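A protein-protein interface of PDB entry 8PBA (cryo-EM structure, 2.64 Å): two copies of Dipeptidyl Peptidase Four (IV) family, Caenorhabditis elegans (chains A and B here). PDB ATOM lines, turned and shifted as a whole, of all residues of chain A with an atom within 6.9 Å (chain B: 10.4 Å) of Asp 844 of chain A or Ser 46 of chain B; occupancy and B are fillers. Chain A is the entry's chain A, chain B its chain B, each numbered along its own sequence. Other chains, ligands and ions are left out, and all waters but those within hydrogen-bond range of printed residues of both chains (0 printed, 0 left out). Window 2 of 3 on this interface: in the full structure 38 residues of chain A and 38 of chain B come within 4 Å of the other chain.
The backbone carbonyl oxygen (O) of Lys 877 of chain A is in hydrogen-bond range of the side-chain hydroxyl (OH) of Tyr 899 of chain B.
The side-chain amino group (NZ) of Lys 877 of chain A is in hydrogen-bond range of the backbone carbonyl oxygen (O) of Glu 840 of chain A (3.1 Å).
The backbone carbonyl oxygen (O) of Leu 842 of chain A is in hydrogen-bond range of the side-chain amino group (NZ) of Lys 877 of chain A, at 2.9 Å.
OD2 of Asp 844 of chain A is in salt-bridge range of NZ of Lys 877 of chain A, 2.9 Å away.
The backbone NH (N) of Ser 46 of chain B sits close to the side-chain hydroxyl (OG) of Ser 44 of chain B (3.2 Å).
The side-chain hydroxyl (OH) of Tyr 899 of chain B sits at hydrogen-bond distance from the guanidinium group (NH1) of Arg 903 of chain B.
Among the printed residues, pairs that only touch across the chains: Asp 844 of chain A with Ser 46 of chain B, Pro 846 of chain A with Tyr 906 of chain B, Gly 876 of chain A with Phe 45 of chain B, Trp 878 of chain A with Phe 45 of chain B, Trp 878 of chain A with Tyr 899 of chain B and Trp 878 of chain A with Arg 903 of chain B.
Of chain B, only Ser 46 comes within 4 Å of Asp 844 of chain A.
Ser 46 of chain B touches one residue of chain A.
No residue of chain B comes within 4 Å of Glu 845 of chain A.
Of the printed residues of chain A, Arg 903 of chain B touches Trp 878.
Printed residues of chain B within 4 Å of Trp 878 of chain A: Phe 45 (3.9 Å), Tyr 899 (3.9 Å) and Arg 903 (3.7 Å).
Of the printed residues of chain B, Lys 877 of chain A touches Tyr 899.
Printed residues of chain B within 4 Å of Gly 876 of chain A: Phe 45 (3.3 Å).
Printed residues of chain A within 4 Å of Phe 45 of chain B: Gly 876 (3.3 Å) and Trp 878 (3.9 Å).
Ile 49 of chain B touches none of the printed residues of chain A.
The nearest residue of chain A that does not touch Ser 46 of chain B is Gly 876 of chain A (5.6 Å).
Of the 12 printed residues of chain A, 5 touch a printed residue of chain B.
Of the 23 printed residues of chain B, 5 touch a printed residue of chain A.
Hydrophobic or aromatic side chains of chain B within 4 Å of the printed part of chain A: Phe 45, Tyr 899 and Tyr 906.
No position is printed for both chains.
Of the 7 pairs that touch across the chains among the printed residues, none has its exchanged pair printed and touching as well.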
ATOM      1  N   GLU A 840      -2.800  -0.235   3.340  1.00  0.00           N
ATOM      2  CA  GLU A 840      -2.953   0.176   1.960  1.00  0.00           C
ATOM      3  C   GLU A 840      -4.211   1.004   1.743  1.00  0.00           C
ATOM      4  O   GLU A 840      -4.290   1.778   0.789  1.00  0.00           O
ATOM      5  CB  GLU A 840      -3.009  -1.050   1.073  1.00  0.00           C
ATOM      6  CG  GLU A 840      -3.169  -0.754  -0.385  1.00  0.00           C
ATOM      7  CD  GLU A 840      -3.076  -1.985  -1.222  1.00  0.00           C
ATOM      8  OE1 GLU A 840      -2.777  -3.020  -0.679  1.00  0.00           O
ATOM      9  OE2 GLU A 840      -3.317  -1.902  -2.403  1.00  0.00           O
ATOM     10  N   LYS A 841      -5.241   0.735   2.537  1.00  0.00           N
ATOM     11  CA  LYS A 841      -6.537   1.374   2.374  1.00  0.00           C
ATOM     12  C   LYS A 841      -6.655   2.649   3.197  1.00  0.00           C
ATOM     13  O   LYS A 841      -7.672   3.337   3.147  1.00  0.00           O
ATOM     14  CB  LYS A 841      -7.647   0.414   2.777  1.00  0.00           C
ATOM     15  CG  LYS A 841      -7.705  -0.883   1.999  1.00  0.00           C
ATOM     16  CD  LYS A 841      -8.076  -0.652   0.554  1.00  0.00           C
ATOM     17  CE  LYS A 841      -8.352  -1.963  -0.158  1.00  0.00           C
ATOM     18  NZ  LYS A 841      -8.719  -1.751  -1.585  1.00  0.00           N
ATOM     19  N   LEU A 842      -5.637   2.950   3.987  1.00  0.00           N
ATOM     20  CA  LEU A 842      -5.668   4.158   4.782  1.00  0.00           C
ATOM     21  C   LEU A 842      -5.616   5.341   3.835  1.00  0.00           C
ATOM     22  O   LEU A 842      -5.096   5.220   2.726  1.00  0.00           O
ATOM     23  CB  LEU A 842      -4.499   4.169   5.782  1.00  0.00           C
ATOM     24  CG  LEU A 842      -4.596   3.159   6.945  1.00  0.00           C
ATOM     25  CD1 LEU A 842      -3.293   3.171   7.725  1.00  0.00           C
ATOM     26  CD2 LEU A 842      -5.766   3.520   7.867  1.00  0.00           C
ATOM     27  N   PRO A 843      -6.178   6.483   4.227  1.00  0.00           N
ATOM     28  CA  PRO A 843      -6.313   7.674   3.424  1.00  0.00           C
ATOM     29  C   PRO A 843      -4.974   8.189   2.945  1.00  0.00           C
ATOM     30  O   PRO A 843      -3.985   8.168   3.677  1.00  0.00           O
ATOM     31  CB  PRO A 843      -6.972   8.653   4.397  1.00  0.00           C
ATOM     32  CG  PRO A 843      -6.759   8.063   5.770  1.00  0.00           C
ATOM     33  CD  PRO A 843      -6.770   6.589   5.557  1.00  0.00           C
ATOM     34  N   ASP A 844      -4.958   8.684   1.715  1.00  0.00           N
ATOM     35  CA  ASP A 844      -3.744   9.217   1.124  1.00  0.00           C
ATOM     36  C   ASP A 844      -3.537  10.653   1.550  1.00  0.00           C
ATOM     37  O   ASP A 844      -2.406  11.133   1.634  1.00  0.00           O
ATOM     38  CB  ASP A 844      -3.842   9.172  -0.392  1.00  0.00           C
ATOM     39  CG  ASP A 844      -3.950   7.776  -0.926  1.00  0.00           C
ATOM     40  OD1 ASP A 844      -4.995   7.445  -1.431  1.00  0.00           O
ATOM     41  OD2 ASP A 844      -2.986   7.040  -0.850  1.00  0.00           O
ATOM     42  N   GLU A 845      -4.632  11.352   1.786  1.00  0.00           N
ATOM     43  CA  GLU A 845      -4.553  12.737   2.178  1.00  0.00           C
ATOM     44  C   GLU A 845      -4.079  12.845   3.613  1.00  0.00           C
ATOM     45  O   GLU A 845      -4.385  11.983   4.434  1.00  0.00           O
ATOM     46  CB  GLU A 845      -5.909  13.401   2.054  1.00  0.00           C
ATOM     47  CG  GLU A 845      -6.524  13.274   0.707  1.00  0.00           C
ATOM     48  CD  GLU A 845      -7.384  12.079   0.606  1.00  0.00           C
ATOM     49  OE1 GLU A 845      -7.292  11.238   1.466  1.00  0.00           O
ATOM     50  OE2 GLU A 845      -8.153  11.996  -0.317  1.00  0.00           O
ATOM     51  N   PRO A 846      -3.392  13.925   3.948  1.00  0.00           N
ATOM     52  CA  PRO A 846      -2.955  14.296   5.268  1.00  0.00           C
ATOM     53  C   PRO A 846      -4.112  14.741   6.141  1.00  0.00           C
ATOM     54  O   PRO A 846      -5.182  15.089   5.647  1.00  0.00           O
ATOM     55  CB  PRO A 846      -1.971  15.422   4.981  1.00  0.00           C
ATOM     56  CG  PRO A 846      -2.419  15.981   3.671  1.00  0.00           C
ATOM     57  CD  PRO A 846      -2.942  14.816   2.899  1.00  0.00           C
ATOM     58  N   ARG A 848      -5.969  13.050   8.008  1.00  0.00           N
ATOM     59  CA  ARG A 848      -7.094  12.136   8.103  1.00  0.00           C
ATOM     60  C   ARG A 848      -6.859  11.066   9.162  1.00  0.00           C
ATOM     61  O   ARG A 848      -7.802  10.605   9.796  1.00  0.00           O
ATOM     62  CB  ARG A 848      -7.418  11.527   6.748  1.00  0.00           C
ATOM     63  CG  ARG A 848      -7.905  12.557   5.743  1.00  0.00           C
ATOM     64  CD  ARG A 848      -8.503  11.980   4.535  1.00  0.00           C
ATOM     65  NE  ARG A 848      -9.744  11.333   4.816  1.00  0.00           N
ATOM     66  CZ  ARG A 848     -10.470  10.644   3.928  1.00  0.00           C
ATOM     67  NH1 ARG A 848     -11.608  10.104   4.294  1.00  0.00           N
ATOM     68  NH2 ARG A 848     -10.050  10.507   2.689  1.00  0.00           N
ATOM     69  N   LYS A 875       4.196   2.188   2.827  1.00  0.00           N
ATOM     70  CA  LYS A 875       3.102   2.414   1.898  1.00  0.00           C
ATOM     71  C   LYS A 875       2.948   3.871   1.488  1.00  0.00           C
ATOM     72  O   LYS A 875       2.230   4.170   0.533  1.00  0.00           O
ATOM     73  CB  LYS A 875       1.799   1.900   2.487  1.00  0.00           C
ATOM     74  CG  LYS A 875       1.775   0.416   2.787  1.00  0.00           C
ATOM     75  CD  LYS A 875       1.854  -0.414   1.543  1.00  0.00           C
ATOM     76  CE  LYS A 875       1.643  -1.875   1.865  1.00  0.00           C
ATOM     77  NZ  LYS A 875       1.777  -2.729   0.661  1.00  0.00           N
ATOM     78  N   GLY A 876       3.647   4.775   2.165  1.00  0.00           N
ATOM     79  CA  GLY A 876       3.565   6.187   1.823  1.00  0.00           C
ATOM     80  C   GLY A 876       2.310   6.845   2.374  1.00  0.00           C
ATOM     81  O   GLY A 876       1.756   7.751   1.756  1.00  0.00           O
ATOM     82  N   LYS A 877       1.798   6.322   3.477  1.00  0.00           N
ATOM     83  CA  LYS A 877       0.594   6.871   4.081  1.00  0.00           C
ATOM     84  C   LYS A 877       0.928   7.872   5.171  1.00  0.00           C
ATOM     85  O   LYS A 877       1.755   7.610   6.038  1.00  0.00           O
ATOM     86  CB  LYS A 877      -0.269   5.754   4.645  1.00  0.00           C
ATOM     87  CG  LYS A 877      -0.656   4.705   3.632  1.00  0.00           C
ATOM     88  CD  LYS A 877      -1.599   5.251   2.592  1.00  0.00           C
ATOM     89  CE  LYS A 877      -2.014   4.186   1.624  1.00  0.00           C
ATOM     90  NZ  LYS A 877      -3.087   4.649   0.721  1.00  0.00           N
ATOM     91  N   TRP A 878       0.263   9.011   5.130  1.00  0.00           N
ATOM     92  CA  TRP A 878       0.461  10.076   6.097  1.00  0.00           C
ATOM     93  C   TRP A 878      -0.215   9.751   7.415  1.00  0.00           C
ATOM     94  O   TRP A 878      -1.302   9.176   7.437  1.00  0.00           O
ATOM     95  CB  TRP A 878      -0.145  11.357   5.551  1.00  0.00           C
ATOM     96  CG  TRP A 878       0.241  12.591   6.261  1.00  0.00           C
ATOM     97  CD1 TRP A 878       1.244  13.407   5.917  1.00  0.00           C
ATOM     98  CD2 TRP A 878      -0.354  13.172   7.425  1.00  0.00           C
ATOM     99  NE1 TRP A 878       1.298  14.459   6.761  1.00  0.00           N
ATOM    100  CE2 TRP A 878       0.329  14.330   7.686  1.00  0.00           C
ATOM    101  CE3 TRP A 878      -1.396  12.805   8.253  1.00  0.00           C
ATOM    102  CZ2 TRP A 878       0.010  15.132   8.731  1.00  0.00           C
ATOM    103  CZ3 TRP A 878      -1.700  13.602   9.320  1.00  0.00           C
ATOM    104  CH2 TRP A 878      -1.020  14.740   9.544  1.00  0.00           C
ATOM    105  N   THR B  42       1.912  24.506  -4.681  1.00  0.00           N
ATOM    106  CA  THR B  42       1.634  23.515  -3.669  1.00  0.00           C
ATOM    107  C   THR B  42       1.330  22.197  -4.342  1.00  0.00           C
ATOM    108  O   THR B  42       0.990  22.167  -5.524  1.00  0.00           O
ATOM    109  CB  THR B  42       0.450  23.954  -2.796  1.00  0.00           C
ATOM    110  OG1 THR B  42      -0.719  24.083  -3.611  1.00  0.00           O
ATOM    111  CG2 THR B  42       0.756  25.288  -2.144  1.00  0.00           C
ATOM    112  N   ARG B  43       1.421  21.111  -3.590  1.00  0.00           N
ATOM    113  CA  ARG B  43       1.053  19.808  -4.125  1.00  0.00           C
ATOM    114  C   ARG B  43       0.718  18.786  -3.051  1.00  0.00           C
ATOM    115  O   ARG B  43       0.969  18.997  -1.866  1.00  0.00           O
ATOM    116  CB  ARG B  43       2.103  19.286  -5.090  1.00  0.00           C
ATOM    117  CG  ARG B  43       3.504  19.389  -4.628  1.00  0.00           C
ATOM    118  CD  ARG B  43       4.429  18.589  -5.470  1.00  0.00           C
ATOM    119  NE  ARG B  43       4.411  18.978  -6.858  1.00  0.00           N
ATOM    120  CZ  ARG B  43       5.119  19.989  -7.383  1.00  0.00           C
ATOM    121  NH1 ARG B  43       5.861  20.751  -6.622  1.00  0.00           N
ATOM    122  NH2 ARG B  43       5.065  20.215  -8.678  1.00  0.00           N
ATOM    123  N   SER B  44       0.074  17.709  -3.483  1.00  0.00           N
ATOM    124  CA  SER B  44      -0.378  16.633  -2.615  1.00  0.00           C
ATOM    125  C   SER B  44       0.752  15.810  -2.045  1.00  0.00           C
ATOM    126  O   SER B  44       1.737  15.527  -2.724  1.00  0.00           O
ATOM    127  CB  SER B  44      -1.318  15.713  -3.360  1.00  0.00           C
ATOM    128  OG  SER B  44      -1.632  14.584  -2.583  1.00  0.00           O
ATOM    129  N   PHE B  45       0.522  15.264  -0.864  1.00  0.00           N
ATOM    130  CA  PHE B  45       1.497  14.399  -0.235  1.00  0.00           C
ATOM    131  C   PHE B  45       1.904  13.278  -1.166  1.00  0.00           C
ATOM    132  O   PHE B  45       3.071  12.896  -1.204  1.00  0.00           O
ATOM    133  CB  PHE B  45       0.957  13.808   1.055  1.00  0.00           C
ATOM    134  CG  PHE B  45       1.943  12.951   1.721  1.00  0.00           C
ATOM    135  CD1 PHE B  45       2.991  13.511   2.380  1.00  0.00           C
ATOM    136  CD2 PHE B  45       1.858  11.589   1.662  1.00  0.00           C
ATOM    137  CE1 PHE B  45       3.939  12.739   2.950  1.00  0.00           C
ATOM    138  CE2 PHE B  45       2.803  10.815   2.254  1.00  0.00           C
ATOM    139  CZ  PHE B  45       3.846  11.394   2.897  1.00  0.00           C
ATOM    140  N   SER B  46       0.943  12.736  -1.905  1.00  0.00           N
ATOM    141  CA  SER B  46       1.229  11.625  -2.801  1.00  0.00           C
ATOM    142  C   SER B  46       2.151  12.056  -3.931  1.00  0.00           C
ATOM    143  O   SER B  46       2.856  11.237  -4.522  1.00  0.00           O
ATOM    144  CB  SER B  46      -0.056  11.078  -3.380  1.00  0.00           C
ATOM    145  OG  SER B  46      -0.838  10.469  -2.391  1.00  0.00           O
ATOM    146  N   GLN B  47       2.134  13.342  -4.246  1.00  0.00           N
ATOM    147  CA  GLN B  47       2.962  13.880  -5.309  1.00  0.00           C
ATOM    148  C   GLN B  47       4.360  14.165  -4.792  1.00  0.00           C
ATOM    149  O   GLN B  47       5.335  14.060  -5.537  1.00  0.00           O
ATOM    150  CB  GLN B  47       2.324  15.140  -5.880  1.00  0.00           C
ATOM    151  CG  GLN B  47       1.012  14.876  -6.595  1.00  0.00           C
ATOM    152  CD  GLN B  47       0.294  16.143  -7.043  1.00  0.00           C
ATOM    153  OE1 GLN B  47      -0.063  17.026  -6.250  1.00  0.00           O
ATOM    154  NE2 GLN B  47       0.063  16.228  -8.346  1.00  0.00           N
ATOM    155  N   LEU B  48       4.464  14.428  -3.492  1.00  0.00           N
ATOM    156  CA  LEU B  48       5.760  14.638  -2.875  1.00  0.00           C
ATOM    157  C   LEU B  48       6.471  13.294  -2.766  1.00  0.00           C
ATOM    158  O   LEU B  48       7.686  13.214  -2.942  1.00  0.00           O
ATOM    159  CB  LEU B  48       5.620  15.262  -1.480  1.00  0.00           C
ATOM    160  CG  LEU B  48       5.478  16.821  -1.358  1.00  0.00           C
ATOM    161  CD1 LEU B  48       6.447  17.553  -2.279  1.00  0.00           C
ATOM    162  CD2 LEU B  48       4.060  17.229  -1.624  1.00  0.00           C
ATOM    163  N   ILE B  49       5.697  12.228  -2.552  1.00  0.00           N
ATOM    164  CA  ILE B  49       6.247  10.878  -2.540  1.00  0.00           C
ATOM    165  C   ILE B  49       6.802  10.513  -3.905  1.00  0.00           C
ATOM    166  O   ILE B  49       7.924  10.017  -4.006  1.00  0.00           O
ATOM    167  CB  ILE B  49       5.185   9.832  -2.139  1.00  0.00           C
ATOM    168  CG1 ILE B  49       4.777   9.964  -0.665  1.00  0.00           C
ATOM    169  CG2 ILE B  49       5.693   8.430  -2.431  1.00  0.00           C
ATOM    170  CD1 ILE B  49       5.816   9.469   0.333  1.00  0.00           C
ATOM    171  N   ASP B  50       6.058  10.817  -4.963  1.00  0.00           N
ATOM    172  CA  ASP B  50       6.535  10.501  -6.301  1.00  0.00           C
ATOM    173  C   ASP B  50       7.736  11.338  -6.671  1.00  0.00           C
ATOM    174  O   ASP B  50       8.624  10.878  -7.389  1.00  0.00           O
ATOM    175  CB  ASP B  50       5.451  10.723  -7.337  1.00  0.00           C
ATOM    176  CG  ASP B  50       4.395   9.671  -7.316  1.00  0.00           C
ATOM    177  OD1 ASP B  50       3.363   9.887  -7.903  1.00  0.00           O
ATOM    178  OD2 ASP B  50       4.632   8.627  -6.762  1.00  0.00           O
ATOM    179  N   HIS B  51       7.770  12.570  -6.187  1.00  0.00           N
ATOM    180  CA  HIS B  51       8.892  13.438  -6.475  1.00  0.00           C
ATOM    181  C   HIS B  51      10.158  12.894  -5.852  1.00  0.00           C
ATOM    182  O   HIS B  51      11.171  12.723  -6.532  1.00  0.00           O
ATOM    183  CB  HIS B  51       8.628  14.843  -5.939  1.00  0.00           C
ATOM    184  CG  HIS B  51       9.760  15.762  -6.119  1.00  0.00           C
ATOM    185  ND1 HIS B  51      10.195  16.167  -7.354  1.00  0.00           N
ATOM    186  CD2 HIS B  51      10.542  16.379  -5.224  1.00  0.00           C
ATOM    187  CE1 HIS B  51      11.209  16.985  -7.206  1.00  0.00           C
ATOM    188  NE2 HIS B  51      11.434  17.136  -5.923  1.00  0.00           N
ATOM    189  N   ALA B  52      10.083  12.551  -4.573  1.00  0.00           N
ATOM    190  CA  ALA B  52      11.240  12.035  -3.869  1.00  0.00           C
ATOM    191  C   ALA B  52      11.674  10.699  -4.452  1.00  0.00           C
ATOM    192  O   ALA B  52      12.866  10.402  -4.522  1.00  0.00           O
ATOM    193  CB  ALA B  52      10.932  11.909  -2.392  1.00  0.00           C
ATOM    194  N   ARG B  53      10.708   9.902  -4.887  1.00  0.00           N
ATOM    195  CA  ARG B  53      11.006   8.592  -5.438  1.00  0.00           C
ATOM    196  C   ARG B  53      11.687   8.672  -6.796  1.00  0.00           C
ATOM    197  O   ARG B  53      12.686   7.988  -7.044  1.00  0.00           O
ATOM    198  CB  ARG B  53       9.726   7.797  -5.565  1.00  0.00           C
ATOM    199  CG  ARG B  53       9.892   6.390  -6.051  1.00  0.00           C
ATOM    200  CD  ARG B  53       8.607   5.665  -6.040  1.00  0.00           C
ATOM    201  NE  ARG B  53       8.068   5.547  -4.699  1.00  0.00           N
ATOM    202  CZ  ARG B  53       8.453   4.627  -3.789  1.00  0.00           C
ATOM    203  NH1 ARG B  53       9.381   3.741  -4.074  1.00  0.00           N
ATOM    204  NH2 ARG B  53       7.914   4.614  -2.587  1.00  0.00           N
ATOM    205  N   SER B  54      11.175   9.536  -7.664  1.00  0.00           N
ATOM    206  CA  SER B  54      11.753   9.704  -8.985  1.00  0.00           C
ATOM    207  C   SER B  54      13.130  10.311  -8.860  1.00  0.00           C
ATOM    208  O   SER B  54      14.059   9.936  -9.577  1.00  0.00           O
ATOM    209  CB  SER B  54      10.873  10.584  -9.842  1.00  0.00           C
ATOM    210  OG  SER B  54      11.410  10.730 -11.127  1.00  0.00           O
ATOM    211  N   LEU B 719      11.511  22.261  -6.348  1.00  0.00           N
ATOM    212  CA  LEU B 719      10.226  22.586  -5.764  1.00  0.00           C
ATOM    213  C   LEU B 719      10.106  24.082  -5.504  1.00  0.00           C
ATOM    214  O   LEU B 719       9.191  24.530  -4.815  1.00  0.00           O
ATOM    215  CB  LEU B 719      10.010  21.796  -4.479  1.00  0.00           C
ATOM    216  CG  LEU B 719       9.994  20.277  -4.631  1.00  0.00           C
ATOM    217  CD1 LEU B 719       9.871  19.669  -3.286  1.00  0.00           C
ATOM    218  CD2 LEU B 719       8.840  19.834  -5.512  1.00  0.00           C
ATOM    219  N   ILE B 898      12.404   8.049   1.164  1.00  0.00           N
ATOM    220  CA  ILE B 898      11.419   8.718   0.327  1.00  0.00           C
ATOM    221  C   ILE B 898      10.303   9.296   1.169  1.00  0.00           C
ATOM    222  O   ILE B 898       9.882  10.433   0.967  1.00  0.00           O
ATOM    223  CB  ILE B 898      10.831   7.740  -0.699  1.00  0.00           C
ATOM    224  CG1 ILE B 898      11.888   7.393  -1.729  1.00  0.00           C
ATOM    225  CG2 ILE B 898       9.574   8.303  -1.346  1.00  0.00           C
ATOM    226  CD1 ILE B 898      11.555   6.214  -2.592  1.00  0.00           C
ATOM    227  N   TYR B 899       9.842   8.519   2.133  1.00  0.00           N
ATOM    228  CA  TYR B 899       8.787   8.969   3.013  1.00  0.00           C
ATOM    229  C   TYR B 899       9.211  10.183   3.807  1.00  0.00           C
ATOM    230  O   TYR B 899       8.450  11.143   3.935  1.00  0.00           O
ATOM    231  CB  TYR B 899       8.395   7.861   3.958  1.00  0.00           C
ATOM    232  CG  TYR B 899       7.263   8.201   4.817  1.00  0.00           C
ATOM    233  CD1 TYR B 899       6.011   8.163   4.312  1.00  0.00           C
ATOM    234  CD2 TYR B 899       7.470   8.530   6.104  1.00  0.00           C
ATOM    235  CE1 TYR B 899       4.957   8.436   5.096  1.00  0.00           C
ATOM    236  CE2 TYR B 899       6.420   8.806   6.895  1.00  0.00           C
ATOM    237  CZ  TYR B 899       5.164   8.748   6.393  1.00  0.00           C
ATOM    238  OH  TYR B 899       4.100   9.021   7.199  1.00  0.00           O
ATOM    239  N   ASP B 901      11.438  12.402   3.079  1.00  0.00           N
ATOM    240  CA  ASP B 901      11.557  13.580   2.257  1.00  0.00           C
ATOM    241  C   ASP B 901      10.191  14.137   1.953  1.00  0.00           C
ATOM    242  O   ASP B 901       9.981  15.345   2.028  1.00  0.00           O
ATOM    243  CB  ASP B 901      12.235  13.245   0.945  1.00  0.00           C
ATOM    244  CG  ASP B 901      13.685  12.918   1.082  1.00  0.00           C
ATOM    245  OD1 ASP B 901      14.266  13.212   2.100  1.00  0.00           O
ATOM    246  OD2 ASP B 901      14.251  12.454   0.113  1.00  0.00           O
ATOM    247  N   ALA B 902       9.232  13.262   1.696  1.00  0.00           N
ATOM    248  CA  ALA B 902       7.906  13.729   1.354  1.00  0.00           C
ATOM    249  C   ALA B 902       7.261  14.484   2.498  1.00  0.00           C
ATOM    250  O   ALA B 902       6.572  15.476   2.273  1.00  0.00           O
ATOM    251  CB  ALA B 902       7.033  12.576   0.936  1.00  0.00           C
ATOM    252  N   ARG B 903       7.522  14.063   3.729  1.00  0.00           N
ATOM    253  CA  ARG B 903       6.917  14.745   4.860  1.00  0.00           C
ATOM    254  C   ARG B 903       7.620  16.026   5.212  1.00  0.00           C
ATOM    255  O   ARG B 903       6.981  16.988   5.634  1.00  0.00           O
ATOM    256  CB  ARG B 903       6.847  13.859   6.071  1.00  0.00           C
ATOM    257  CG  ARG B 903       5.862  12.794   5.923  1.00  0.00           C
ATOM    258  CD  ARG B 903       5.519  12.186   7.140  1.00  0.00           C
ATOM    259  NE  ARG B 903       4.760  13.050   7.967  1.00  0.00           N
ATOM    260  CZ  ARG B 903       3.949  12.617   8.920  1.00  0.00           C
ATOM    261  NH1 ARG B 903       3.771  11.338   9.094  1.00  0.00           N
ATOM    262  NH2 ARG B 903       3.317  13.456   9.692  1.00  0.00           N
ATOM    263  N   MET B 905       8.957  17.930   3.045  1.00  0.00           N
ATOM    264  CA  MET B 905       8.588  18.829   1.973  1.00  0.00           C
ATOM    265  C   MET B 905       7.136  19.249   2.074  1.00  0.00           C
ATOM    266  O   MET B 905       6.815  20.424   1.895  1.00  0.00           O
ATOM    267  CB  MET B 905       8.872  18.151   0.656  1.00  0.00           C
ATOM    268  CG  MET B 905      10.350  17.944   0.428  1.00  0.00           C
ATOM    269  SD  MET B 905      10.770  17.300  -1.180  1.00  0.00           S
ATOM    270  CE  MET B 905       9.983  15.708  -1.251  1.00  0.00           C
ATOM    271  N   TYR B 906       6.271  18.318   2.450  1.00  0.00           N
ATOM    272  CA  TYR B 906       4.868  18.636   2.613  1.00  0.00           C
ATOM    273  C   TYR B 906       4.704  19.629   3.744  1.00  0.00           C
ATOM    274  O   TYR B 906       4.008  20.635   3.613  1.00  0.00           O
ATOM    275  CB  TYR B 906       4.058  17.381   2.899  1.00  0.00           C
ATOM    276  CG  TYR B 906       2.609  17.649   2.971  1.00  0.00           C
ATOM    277  CD1 TYR B 906       1.854  17.594   1.830  1.00  0.00           C
ATOM    278  CD2 TYR B 906       2.053  18.059   4.148  1.00  0.00           C
ATOM    279  CE1 TYR B 906       0.553  17.965   1.862  1.00  0.00           C
ATOM    280  CE2 TYR B 906       0.754  18.440   4.184  1.00  0.00           C
ATOM    281  CZ  TYR B 906       0.011  18.415   3.043  1.00  0.00           C
ATOM    282  OH  TYR B 906      -1.287  18.846   3.071  1.00  0.00           O
ATOM    283  N   GLN B 909       5.636  23.179   2.935  1.00  0.00           N
ATOM    284  CA  GLN B 909       4.674  23.948   2.154  1.00  0.00           C
ATOM    285  C   GLN B 909       3.641  24.577   3.045  1.00  0.00           C
ATOM    286  O   GLN B 909       3.245  25.722   2.845  1.00  0.00           O
ATOM    287  CB  GLN B 909       3.894  23.079   1.179  1.00  0.00           C
ATOM    288  CG  GLN B 909       4.673  22.536   0.088  1.00  0.00           C
ATOM    289  CD  GLN B 909       3.821  21.822  -0.935  1.00  0.00           C
ATOM    290  OE1 GLN B 909       2.591  21.885  -0.941  1.00  0.00           O
ATOM    291  NE2 GLN B 909       4.492  21.118  -1.824  1.00  0.00           N
ATOM    292  N   GLN B 910       3.231  23.842   4.059  1.00  0.00           N
ATOM    293  CA  GLN B 910       2.162  24.315   4.906  1.00  0.00           C
ATOM    294  C   GLN B 910       2.681  25.417   5.803  1.00  0.00           C
ATOM    295  O   GLN B 910       1.956  26.343   6.163  1.00  0.00           O
ATOM    296  CB  GLN B 910       1.626  23.166   5.741  1.00  0.00           C
ATOM    297  CG  GLN B 910       1.157  21.983   4.924  1.00  0.00           C
ATOM    298  CD  GLN B 910       0.135  22.334   3.903  1.00  0.00           C
ATOM    299  OE1 GLN B 910      -0.897  22.926   4.213  1.00  0.00           O
ATOM    300  NE2 GLN B 910       0.408  21.981   2.662  1.00  0.00           N
